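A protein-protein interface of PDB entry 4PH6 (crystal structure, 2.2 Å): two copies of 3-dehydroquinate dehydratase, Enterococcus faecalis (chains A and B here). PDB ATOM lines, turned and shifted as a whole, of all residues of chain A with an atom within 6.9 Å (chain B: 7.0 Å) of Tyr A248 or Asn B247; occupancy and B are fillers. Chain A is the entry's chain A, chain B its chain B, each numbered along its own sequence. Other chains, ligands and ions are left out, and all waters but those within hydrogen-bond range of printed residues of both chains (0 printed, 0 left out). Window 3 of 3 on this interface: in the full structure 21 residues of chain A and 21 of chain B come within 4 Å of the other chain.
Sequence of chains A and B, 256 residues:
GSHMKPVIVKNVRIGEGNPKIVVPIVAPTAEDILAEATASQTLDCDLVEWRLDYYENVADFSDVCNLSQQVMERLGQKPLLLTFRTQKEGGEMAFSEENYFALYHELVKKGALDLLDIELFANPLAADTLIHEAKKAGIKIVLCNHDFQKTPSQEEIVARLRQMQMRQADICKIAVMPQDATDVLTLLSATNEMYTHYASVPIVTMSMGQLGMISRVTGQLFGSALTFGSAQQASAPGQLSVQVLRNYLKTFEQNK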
ATOM      1  N   VAL A 217       6.040 -15.886  -8.562  1.00  0.00           N
ATOM      2  CA  VAL A 217       5.881 -16.926  -9.570  1.00  0.00           C
ATOM      3  C   VAL A 217       4.519 -16.911 -10.269  1.00  0.00           C
ATOM      4  O   VAL A 217       4.281 -17.690 -11.206  1.00  0.00           O
ATOM      5  CB  VAL A 217       6.114 -18.321  -8.953  1.00  0.00           C
ATOM      6  CG1 VAL A 217       7.469 -18.359  -8.237  1.00  0.00           C
ATOM      7  CG2 VAL A 217       4.971 -18.696  -8.002  1.00  0.00           C
ATOM      8  N   LEU A 240      13.998 -16.497  -4.223  1.00  0.00           N
ATOM      9  CA  LEU A 240      14.100 -17.649  -5.113  1.00  0.00           C
ATOM     10  C   LEU A 240      15.185 -17.492  -6.182  1.00  0.00           C
ATOM     11  O   LEU A 240      15.247 -16.485  -6.893  1.00  0.00           O
ATOM     12  CB  LEU A 240      12.746 -17.931  -5.780  1.00  0.00           C
ATOM     13  CG  LEU A 240      11.659 -18.483  -4.843  1.00  0.00           C
ATOM     14  CD1 LEU A 240      10.417 -18.897  -5.627  1.00  0.00           C
ATOM     15  CD2 LEU A 240      12.182 -19.647  -4.002  1.00  0.00           C
ATOM     16  N   GLN A 243      17.249 -20.272 -11.380  1.00  0.00           N
ATOM     17  CA  GLN A 243      16.936 -21.587 -11.950  1.00  0.00           C
ATOM     18  C   GLN A 243      15.587 -22.135 -11.458  1.00  0.00           C
ATOM     19  O   GLN A 243      14.795 -22.655 -12.251  1.00  0.00           O
ATOM     20  CB  GLN A 243      18.042 -22.610 -11.630  1.00  0.00           C
ATOM     21  CG  GLN A 243      17.623 -24.065 -11.885  1.00  0.00           C
ATOM     22  CD  GLN A 243      18.638 -25.096 -11.381  1.00  0.00           C
ATOM     23  OE1 GLN A 243      19.190 -24.960 -10.290  1.00  0.00           O
ATOM     24  NE2 GLN A 243      18.862 -26.144 -12.170  1.00  0.00           N
ATOM     25  N   VAL A 244      15.349 -22.045 -10.151  1.00  0.00           N
ATOM     26  CA  VAL A 244      14.100 -22.512  -9.555  1.00  0.00           C
ATOM     27  C   VAL A 244      12.943 -21.699 -10.112  1.00  0.00           C
ATOM     28  O   VAL A 244      11.832 -22.204 -10.320  1.00  0.00           O
ATOM     29  CB  VAL A 244      14.130 -22.397  -8.002  1.00  0.00           C
ATOM     30  CG1 VAL A 244      12.742 -22.543  -7.411  1.00  0.00           C
ATOM     31  CG2 VAL A 244      15.087 -23.412  -7.393  1.00  0.00           C
ATOM     32  N   LEU A 245      13.229 -20.428 -10.366  1.00  0.00           N
ATOM     33  CA  LEU A 245      12.227 -19.478 -10.802  1.00  0.00           C
ATOM     34  C   LEU A 245      11.659 -19.844 -12.173  1.00  0.00           C
ATOM     35  O   LEU A 245      10.442 -19.903 -12.363  1.00  0.00           O
ATOM     36  CB  LEU A 245      12.840 -18.082 -10.834  1.00  0.00           C
ATOM     37  CG  LEU A 245      11.926 -16.907 -10.553  1.00  0.00           C
ATOM     38  CD1 LEU A 245      10.986 -17.214  -9.368  1.00  0.00           C
ATOM     39  CD2 LEU A 245      12.786 -15.672 -10.280  1.00  0.00           C
ATOM     40  N   ARG A 246      12.553 -20.090 -13.125  1.00  0.00           N
ATOM     41  CA  ARG A 246      12.142 -20.520 -14.453  1.00  0.00           C
ATOM     42  C   ARG A 246      11.305 -21.794 -14.364  1.00  0.00           C
ATOM     43  O   ARG A 246      10.248 -21.884 -14.982  1.00  0.00           O
ATOM     44  CB  ARG A 246      13.353 -20.744 -15.355  1.00  0.00           C
ATOM     45  CG  ARG A 246      12.975 -21.007 -16.797  1.00  0.00           C
ATOM     46  CD  ARG A 246      12.635 -19.719 -17.527  1.00  0.00           C
ATOM     47  NE  ARG A 246      13.841 -19.006 -17.937  1.00  0.00           N
ATOM     48  CZ  ARG A 246      13.855 -17.754 -18.380  1.00  0.00           C
ATOM     49  NH1 ARG A 246      12.729 -17.067 -18.457  1.00  0.00           N
ATOM     50  NH2 ARG A 246      14.999 -17.186 -18.735  1.00  0.00           N
ATOM     51  N   ASN A 247      11.779 -22.766 -13.585  1.00  0.00           N
ATOM     52  CA  ASN A 247      11.070 -24.030 -13.424  1.00  0.00           C
ATOM     53  C   ASN A 247       9.687 -23.796 -12.831  1.00  0.00           C
ATOM     54  O   ASN A 247       8.698 -24.360 -13.293  1.00  0.00           O
ATOM     55  CB  ASN A 247      11.849 -25.001 -12.528  1.00  0.00           C
ATOM     56  CG  ASN A 247      12.956 -25.738 -13.261  1.00  0.00           C
ATOM     57  OD1 ASN A 247      13.051 -25.708 -14.491  1.00  0.00           O
ATOM     58  ND2 ASN A 247      13.796 -26.431 -12.496  1.00  0.00           N
ATOM     59  N   TYR A 248       9.624 -22.952 -11.809  1.00  0.00           N
ATOM     60  CA  TYR A 248       8.359 -22.683 -11.148  1.00  0.00           C
ATOM     61  C   TYR A 248       7.408 -21.926 -12.059  1.00  0.00           C
ATOM     62  O   TYR A 248       6.212 -22.188 -12.048  1.00  0.00           O
ATOM     63  CB  TYR A 248       8.580 -21.919  -9.846  1.00  0.00           C
ATOM     64  CG  TYR A 248       8.877 -22.838  -8.676  1.00  0.00           C
ATOM     65  CD1 TYR A 248       8.242 -22.664  -7.452  1.00  0.00           C
ATOM     66  CD2 TYR A 248       9.773 -23.896  -8.802  1.00  0.00           C
ATOM     67  CE1 TYR A 248       8.503 -23.502  -6.385  1.00  0.00           C
ATOM     68  CE2 TYR A 248      10.039 -24.740  -7.736  1.00  0.00           C
ATOM     69  CZ  TYR A 248       9.402 -24.539  -6.525  1.00  0.00           C
ATOM     70  OH  TYR A 248       9.656 -25.371  -5.454  1.00  0.00           O
ATOM     71  N   LEU A 249       7.934 -21.012 -12.866  1.00  0.00           N
ATOM     72  CA  LEU A 249       7.104 -20.296 -13.826  1.00  0.00           C
ATOM     73  C   LEU A 249       6.473 -21.242 -14.837  1.00  0.00           C
ATOM     74  O   LEU A 249       5.324 -21.059 -15.234  1.00  0.00           O
ATOM     75  CB  LEU A 249       7.919 -19.230 -14.560  1.00  0.00           C
ATOM     76  CG  LEU A 249       8.333 -18.002 -13.746  1.00  0.00           C
ATOM     77  CD1 LEU A 249       9.137 -17.050 -14.602  1.00  0.00           C
ATOM     78  CD2 LEU A 249       7.112 -17.318 -13.168  1.00  0.00           C
ATOM     79  N   LYS A 250       7.225 -22.252 -15.258  1.00  0.00           N
ATOM     80  CA  LYS A 250       6.697 -23.186 -16.248  1.00  0.00           C
ATOM     81  C   LYS A 250       5.604 -24.040 -15.608  1.00  0.00           C
ATOM     82  O   LYS A 250       4.580 -24.297 -16.237  1.00  0.00           O
ATOM     83  CB  LYS A 250       7.800 -24.072 -16.852  1.00  0.00           C
ATOM     84  CG  LYS A 250       7.686 -25.552 -16.536  1.00  0.00           C
ATOM     85  CD  LYS A 250       8.673 -26.430 -17.294  1.00  0.00           C
ATOM     86  CE  LYS A 250       8.336 -27.912 -17.141  1.00  0.00           C
ATOM     87  NZ  LYS A 250       8.472 -28.366 -15.710  1.00  0.00           N
ATOM     88  N   THR A 251       5.798 -24.453 -14.352  1.00  0.00           N
ATOM     89  CA  THR A 251       4.781 -25.244 -13.658  1.00  0.00           C
ATOM     90  C   THR A 251       3.465 -24.465 -13.584  1.00  0.00           C
ATOM     91  O   THR A 251       2.397 -25.013 -13.852  1.00  0.00           O
ATOM     92  CB  THR A 251       5.220 -25.641 -12.235  1.00  0.00           C
ATOM     93  OG1 THR A 251       6.269 -26.612 -12.298  1.00  0.00           O
ATOM     94  CG2 THR A 251       4.041 -26.227 -11.438  1.00  0.00           C
ATOM     95  N   PHE A 252       3.529 -23.188 -13.224  1.00  0.00           N
ATOM     96  CA  PHE A 252       2.297 -22.424 -13.079  1.00  0.00           C
ATOM     97  C   PHE A 252       1.927 -21.677 -14.357  1.00  0.00           C
ATOM     98  O   PHE A 252       1.100 -20.774 -14.329  1.00  0.00           O
ATOM     99  CB  PHE A 252       2.401 -21.455 -11.904  1.00  0.00           C
ATOM    100  CG  PHE A 252       2.519 -22.140 -10.569  1.00  0.00           C
ATOM    101  CD1 PHE A 252       1.501 -22.958 -10.104  1.00  0.00           C
ATOM    102  CD2 PHE A 252       3.643 -21.964  -9.773  1.00  0.00           C
ATOM    103  CE1 PHE A 252       1.600 -23.597  -8.878  1.00  0.00           C
ATOM    104  CE2 PHE A 252       3.748 -22.606  -8.535  1.00  0.00           C
ATOM    105  CZ  PHE A 252       2.725 -23.418  -8.090  1.00  0.00           C
ATOM    106  N   GLU A 253       2.521 -22.081 -15.475  1.00  0.00           N
ATOM    107  CA  GLU A 253       2.232 -21.463 -16.764  1.00  0.00           C
ATOM    108  C   GLU A 253       0.780 -21.655 -17.216  1.00  0.00           C
ATOM    109  O   GLU A 253       0.218 -22.745 -17.072  1.00  0.00           O
ATOM    110  CB  GLU A 253       3.179 -22.024 -17.827  1.00  0.00           C
ATOM    111  CG  GLU A 253       3.002 -21.432 -19.198  1.00  0.00           C
ATOM    112  CD  GLU A 253       3.975 -22.018 -20.199  1.00  0.00           C
ATOM    113  OE1 GLU A 253       5.009 -22.566 -19.760  1.00  0.00           O
ATOM    114  OE2 GLU A 253       3.701 -21.929 -21.419  1.00  0.00           O
ATOM    115  N   ILE B  21      -0.470 -33.901   2.296  1.00  0.00           N
ATOM    116  CA  ILE B  21      -0.690 -34.286   0.908  1.00  0.00           C
ATOM    117  C   ILE B  21      -1.571 -35.530   0.790  1.00  0.00           C
ATOM    118  O   ILE B  21      -1.319 -36.545   1.425  1.00  0.00           O
ATOM    119  CB  ILE B  21       0.657 -34.519   0.187  1.00  0.00           C
ATOM    120  CG1 ILE B  21       1.458 -33.215   0.151  1.00  0.00           C
ATOM    121  CG2 ILE B  21       0.446 -35.026  -1.203  1.00  0.00           C
ATOM    122  CD1 ILE B  21       2.794 -33.308  -0.580  1.00  0.00           C
ATOM    123  N   ASP B  44       5.608 -39.909  -1.696  1.00  0.00           N
ATOM    124  CA  ASP B  44       5.822 -38.866  -0.704  1.00  0.00           C
ATOM    125  C   ASP B  44       4.505 -38.144  -0.380  1.00  0.00           C
ATOM    126  O   ASP B  44       4.289 -37.014  -0.798  1.00  0.00           O
ATOM    127  CB  ASP B  44       6.881 -37.882  -1.191  1.00  0.00           C
ATOM    128  CG  ASP B  44       7.374 -36.960  -0.086  1.00  0.00           C
ATOM    129  OD1 ASP B  44       8.156 -36.038  -0.397  1.00  0.00           O
ATOM    130  OD2 ASP B  44       6.988 -37.150   1.093  1.00  0.00           O
ATOM    131  N   VAL B 217      -0.554 -25.055  -3.523  1.00  0.00           N
ATOM    132  CA  VAL B 217       0.716 -24.953  -2.807  1.00  0.00           C
ATOM    133  C   VAL B 217       0.724 -23.818  -1.765  1.00  0.00           C
ATOM    134  O   VAL B 217       1.721 -23.590  -1.090  1.00  0.00           O
ATOM    135  CB  VAL B 217       1.897 -24.755  -3.790  1.00  0.00           C
ATOM    136  CG1 VAL B 217       1.952 -25.900  -4.788  1.00  0.00           C
ATOM    137  CG2 VAL B 217       1.796 -23.395  -4.524  1.00  0.00           C
ATOM    138  N   VAL B 242       2.605 -35.847  -6.522  1.00  0.00           N
ATOM    139  CA  VAL B 242       2.938 -35.806  -5.099  1.00  0.00           C
ATOM    140  C   VAL B 242       4.408 -35.449  -4.850  1.00  0.00           C
ATOM    141  O   VAL B 242       4.722 -34.739  -3.887  1.00  0.00           O
ATOM    142  CB  VAL B 242       2.597 -37.148  -4.403  1.00  0.00           C
ATOM    143  CG1 VAL B 242       1.098 -37.226  -4.106  1.00  0.00           C
ATOM    144  CG2 VAL B 242       3.036 -38.326  -5.259  1.00  0.00           C
ATOM    145  N   GLN B 243       5.299 -35.925  -5.716  1.00  0.00           N
ATOM    146  CA  GLN B 243       6.707 -35.532  -5.676  1.00  0.00           C
ATOM    147  C   GLN B 243       6.911 -34.015  -5.742  1.00  0.00           C
ATOM    148  O   GLN B 243       7.573 -33.427  -4.876  1.00  0.00           O
ATOM    149  CB  GLN B 243       7.476 -36.179  -6.825  1.00  0.00           C
ATOM    150  CG  GLN B 243       8.939 -35.761  -6.849  1.00  0.00           C
ATOM    151  CD  GLN B 243       9.722 -36.370  -7.998  1.00  0.00           C
ATOM    152  OE1 GLN B 243       9.331 -36.246  -9.155  1.00  0.00           O
ATOM    153  NE2 GLN B 243      10.852 -36.986  -7.692  1.00  0.00           N
ATOM    154  N   VAL B 244       6.345 -33.396  -6.773  1.00  0.00           N
ATOM    155  CA  VAL B 244       6.469 -31.961  -7.000  1.00  0.00           C
ATOM    156  C   VAL B 244       5.841 -31.161  -5.867  1.00  0.00           C
ATOM    157  O   VAL B 244       6.370 -30.126  -5.443  1.00  0.00           O
ATOM    158  CB  VAL B 244       5.804 -31.558  -8.344  1.00  0.00           C
ATOM    159  CG1 VAL B 244       5.643 -30.056  -8.449  1.00  0.00           C
ATOM    160  CG2 VAL B 244       6.604 -32.100  -9.514  1.00  0.00           C
ATOM    161  N   LEU B 245       4.712 -31.664  -5.375  1.00  0.00           N
ATOM    162  CA  LEU B 245       3.896 -30.948  -4.411  1.00  0.00           C
ATOM    163  C   LEU B 245       4.636 -30.688  -3.107  1.00  0.00           C
ATOM    164  O   LEU B 245       4.682 -29.553  -2.621  1.00  0.00           O
ATOM    165  CB  LEU B 245       2.622 -31.739  -4.142  1.00  0.00           C
ATOM    166  CG  LEU B 245       1.354 -30.996  -3.739  1.00  0.00           C
ATOM    167  CD1 LEU B 245       1.203 -29.700  -4.536  1.00  0.00           C
ATOM    168  CD2 LEU B 245       0.164 -31.924  -3.983  1.00  0.00           C
ATOM    169  N   ARG B 246       5.234 -31.736  -2.554  1.00  0.00           N
ATOM    170  CA  ARG B 246       5.976 -31.597  -1.321  1.00  0.00           C
ATOM    171  C   ARG B 246       7.120 -30.599  -1.490  1.00  0.00           C
ATOM    172  O   ARG B 246       7.276 -29.687  -0.673  1.00  0.00           O
ATOM    173  CB  ARG B 246       6.510 -32.946  -0.859  1.00  0.00           C
ATOM    174  CG  ARG B 246       7.182 -32.903   0.485  1.00  0.00           C
ATOM    175  CD  ARG B 246       6.617 -33.986   1.396  1.00  0.00           C
ATOM    176  NE  ARG B 246       5.420 -33.593   2.131  1.00  0.00           N
ATOM    177  CZ  ARG B 246       4.577 -34.455   2.694  1.00  0.00           C
ATOM    178  NH1 ARG B 246       3.523 -34.004   3.355  1.00  0.00           N
ATOM    179  NH2 ARG B 246       4.780 -35.762   2.588  1.00  0.00           N
ATOM    180  N   ASN B 247       7.912 -30.775  -2.547  1.00  0.00           N
ATOM    181  CA  ASN B 247       8.983 -29.839  -2.863  1.00  0.00           C
ATOM    182  C   ASN B 247       8.456 -28.401  -2.888  1.00  0.00           C
ATOM    183  O   ASN B 247       9.049 -27.500  -2.301  1.00  0.00           O
ATOM    184  CB  ASN B 247       9.635 -30.175  -4.218  1.00  0.00           C
ATOM    185  CG  ASN B 247      10.610 -31.352  -4.141  1.00  0.00           C
ATOM    186  OD1 ASN B 247      11.075 -31.735  -3.059  1.00  0.00           O
ATOM    187  ND2 ASN B 247      10.943 -31.912  -5.305  1.00  0.00           N
ATOM    188  N   TYR B 248       7.324 -28.204  -3.552  1.00  0.00           N
ATOM    189  CA  TYR B 248       6.745 -26.874  -3.684  1.00  0.00           C
ATOM    190  C   TYR B 248       6.207 -26.330  -2.371  1.00  0.00           C
ATOM    191  O   TYR B 248       6.260 -25.131  -2.136  1.00  0.00           O
ATOM    192  CB  TYR B 248       5.639 -26.885  -4.731  1.00  0.00           C
ATOM    193  CG  TYR B 248       6.139 -26.679  -6.149  1.00  0.00           C
ATOM    194  CD1 TYR B 248       5.614 -25.673  -6.953  1.00  0.00           C
ATOM    195  CD2 TYR B 248       7.150 -27.473  -6.674  1.00  0.00           C
ATOM    196  CE1 TYR B 248       6.077 -25.472  -8.253  1.00  0.00           C
ATOM    197  CE2 TYR B 248       7.616 -27.283  -7.965  1.00  0.00           C
ATOM    198  CZ  TYR B 248       7.076 -26.287  -8.753  1.00  0.00           C
ATOM    199  OH  TYR B 248       7.543 -26.109 -10.043  1.00  0.00           O
ATOM    200  N   LEU B 249       5.687 -27.208  -1.517  1.00  0.00           N
ATOM    201  CA  LEU B 249       5.209 -26.788  -0.206  1.00  0.00           C
ATOM    202  C   LEU B 249       6.366 -26.310   0.669  1.00  0.00           C
ATOM    203  O   LEU B 249       6.230 -25.333   1.406  1.00  0.00           O
ATOM    204  CB  LEU B 249       4.458 -27.922   0.492  1.00  0.00           C
ATOM    205  CG  LEU B 249       3.115 -28.326  -0.128  1.00  0.00           C
ATOM    206  CD1 LEU B 249       2.542 -29.524   0.578  1.00  0.00           C
ATOM    207  CD2 LEU B 249       2.116 -27.178  -0.084  1.00  0.00           C
ATOM    208  N   LYS B 250       7.499 -27.003   0.591  1.00  0.00           N
ATOM    209  CA  LYS B 250       8.677 -26.610   1.355  1.00  0.00           C
ATOM    210  C   LYS B 250       9.216 -25.257   0.896  1.00  0.00           C
ATOM    211  O   LYS B 250       9.590 -24.432   1.725  1.00  0.00           O
ATOM    212  CB  LYS B 250       9.780 -27.682   1.264  1.00  0.00           C
ATOM    213  CG  LYS B 250       9.302 -29.087   1.617  1.00  0.00           C
ATOM    214  CD  LYS B 250      10.394 -30.139   1.445  1.00  0.00           C
ATOM    215  CE  LYS B 250      10.354 -31.162   2.575  1.00  0.00           C
ATOM    216  NZ  LYS B 250      11.105 -32.397   2.230  1.00  0.00           N
ATOM    217  N   THR B 251       9.231 -25.021  -0.412  1.00  0.00           N
ATOM    218  CA  THR B 251       9.700 -23.743  -0.947  1.00  0.00           C
ATOM    219  C   THR B 251       8.887 -22.549  -0.425  1.00  0.00           C
ATOM    220  O   THR B 251       9.457 -21.526  -0.045  1.00  0.00           O
ATOM    221  CB  THR B 251       9.680 -23.738  -2.490  1.00  0.00           C
ATOM    222  OG1 THR B 251      10.698 -24.612  -2.986  1.00  0.00           O
ATOM    223  CG2 THR B 251       9.935 -22.340  -3.032  1.00  0.00           C
ATOM    224  N   PHE B 252       7.564 -22.676  -0.379  1.00  0.00           N
ATOM    225  CA  PHE B 252       6.721 -21.563   0.065  1.00  0.00           C
ATOM    226  C   PHE B 252       6.333 -21.672   1.534  1.00  0.00           C
ATOM    227  O   PHE B 252       5.368 -21.040   1.974  1.00  0.00           O
ATOM    228  CB  PHE B 252       5.448 -21.469  -0.785  1.00  0.00           C
ATOM    229  CG  PHE B 252       5.708 -21.197  -2.239  1.00  0.00           C
ATOM    230  CD1 PHE B 252       6.255 -19.993  -2.646  1.00  0.00           C
ATOM    231  CD2 PHE B 252       5.395 -22.141  -3.203  1.00  0.00           C
ATOM    232  CE1 PHE B 252       6.495 -19.743  -3.981  1.00  0.00           C
ATOM    233  CE2 PHE B 252       5.630 -21.885  -4.546  1.00  0.00           C
ATOM    234  CZ  PHE B 252       6.181 -20.694  -4.926  1.00  0.00           C
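The side-chain hydroxyl of Thr B251 is in hydrogen-bond range of the side-chain hydroxyl of Tyr A248 (2.8 Å). OG1 of Thr A251 is in hydrogen-bond range of OH of Tyr B248, 2.6 Å away.
O of Asn A247 is in hydrogen-bond range of OG1 of Thr A251 (3.5 Å). The backbone carbonyl oxygen (O) of Asn B247 sits at hydrogen-bond distance from the side-chain hydroxyl (OG1) of Thr B251 (3.4 Å).
Among the printed residues, merely in contact across the chains: Val A217 with Phe B252, Leu A240 with Thr B251, Asn A247 with Tyr B248, Tyr A248 with Asn B247, Tyr A248 with Tyr B248, Tyr A248 with Phe B252, Phe A252 with Val B217 and Phe A252 with Tyr B248.
Of the printed residues of chain B, Val A217 touches Phe B252 (3.9 Å). Of the printed residues of chain B, Leu A240 touches Thr B251 (3.6 Å). Tyr A248 touches just these residues of chain B: Asn B247 (3.9 Å), Tyr B248 (3.4 Å), Thr B251 (2.8 Å) and Phe B252 (3.8 Å). Of the printed residues of chain B, Thr A251 touches Tyr B248 (2.6 Å). Arg B246 touches none of the printed residues of chain A. Of chain A, only Tyr A248 (3.9 Å) comes within 4 Å of Asn B247. Printed residues of chain A within 4 Å of Thr B251: Leu A240 and Tyr A248. Printed residues of chain A within 4 Å of Phe B252: Val A217 (3.9 Å) and Tyr A248 (3.8 Å). The nearest printed residue of chain A that does not touch Asn B247 is Val A244 (8.0 Å).
Of the 14 printed residues of chain B, 5 touch a printed residue of chain A. Hydrophobic or aromatic side chains of chain B that line the printed part of chain A: Val B217, Tyr B248 and Phe B252. Of the 13 printed residues of chain A, 6 touch a printed residue of chain B. Hydrophobic or aromatic side chains of chain A that line the printed part of chain B: Val A217, Leu A240, Tyr A248 and Phe A252. Among the printed residues, 10 pairs touch across the chains. Among the printed residues, no Asp or Glu carboxylate lies within 4 Å of a Lys or Arg side-chain nitrogen of the other chain.
Val A217 touches Phe B252, and with the chains exchanged Phe A252 touches Val B217. Asn A247 touches Tyr B248, and with the chains exchanged Tyr A248 touches Asn B247. Tyr A248 touches Thr B251, and with the chains exchanged Thr A251 touches Tyr B248. Tyr A248 touches Phe B252, and with the chains exchanged Phe A252 touches Tyr B248. Positions printed for both chains: 217, 243, 244, 245, 246, 247, 248, 249, 250, 251 and 252. Of the 10 pairs that touch across the chains among the printed residues, 9 have their exchanged pair printed and touching as well.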
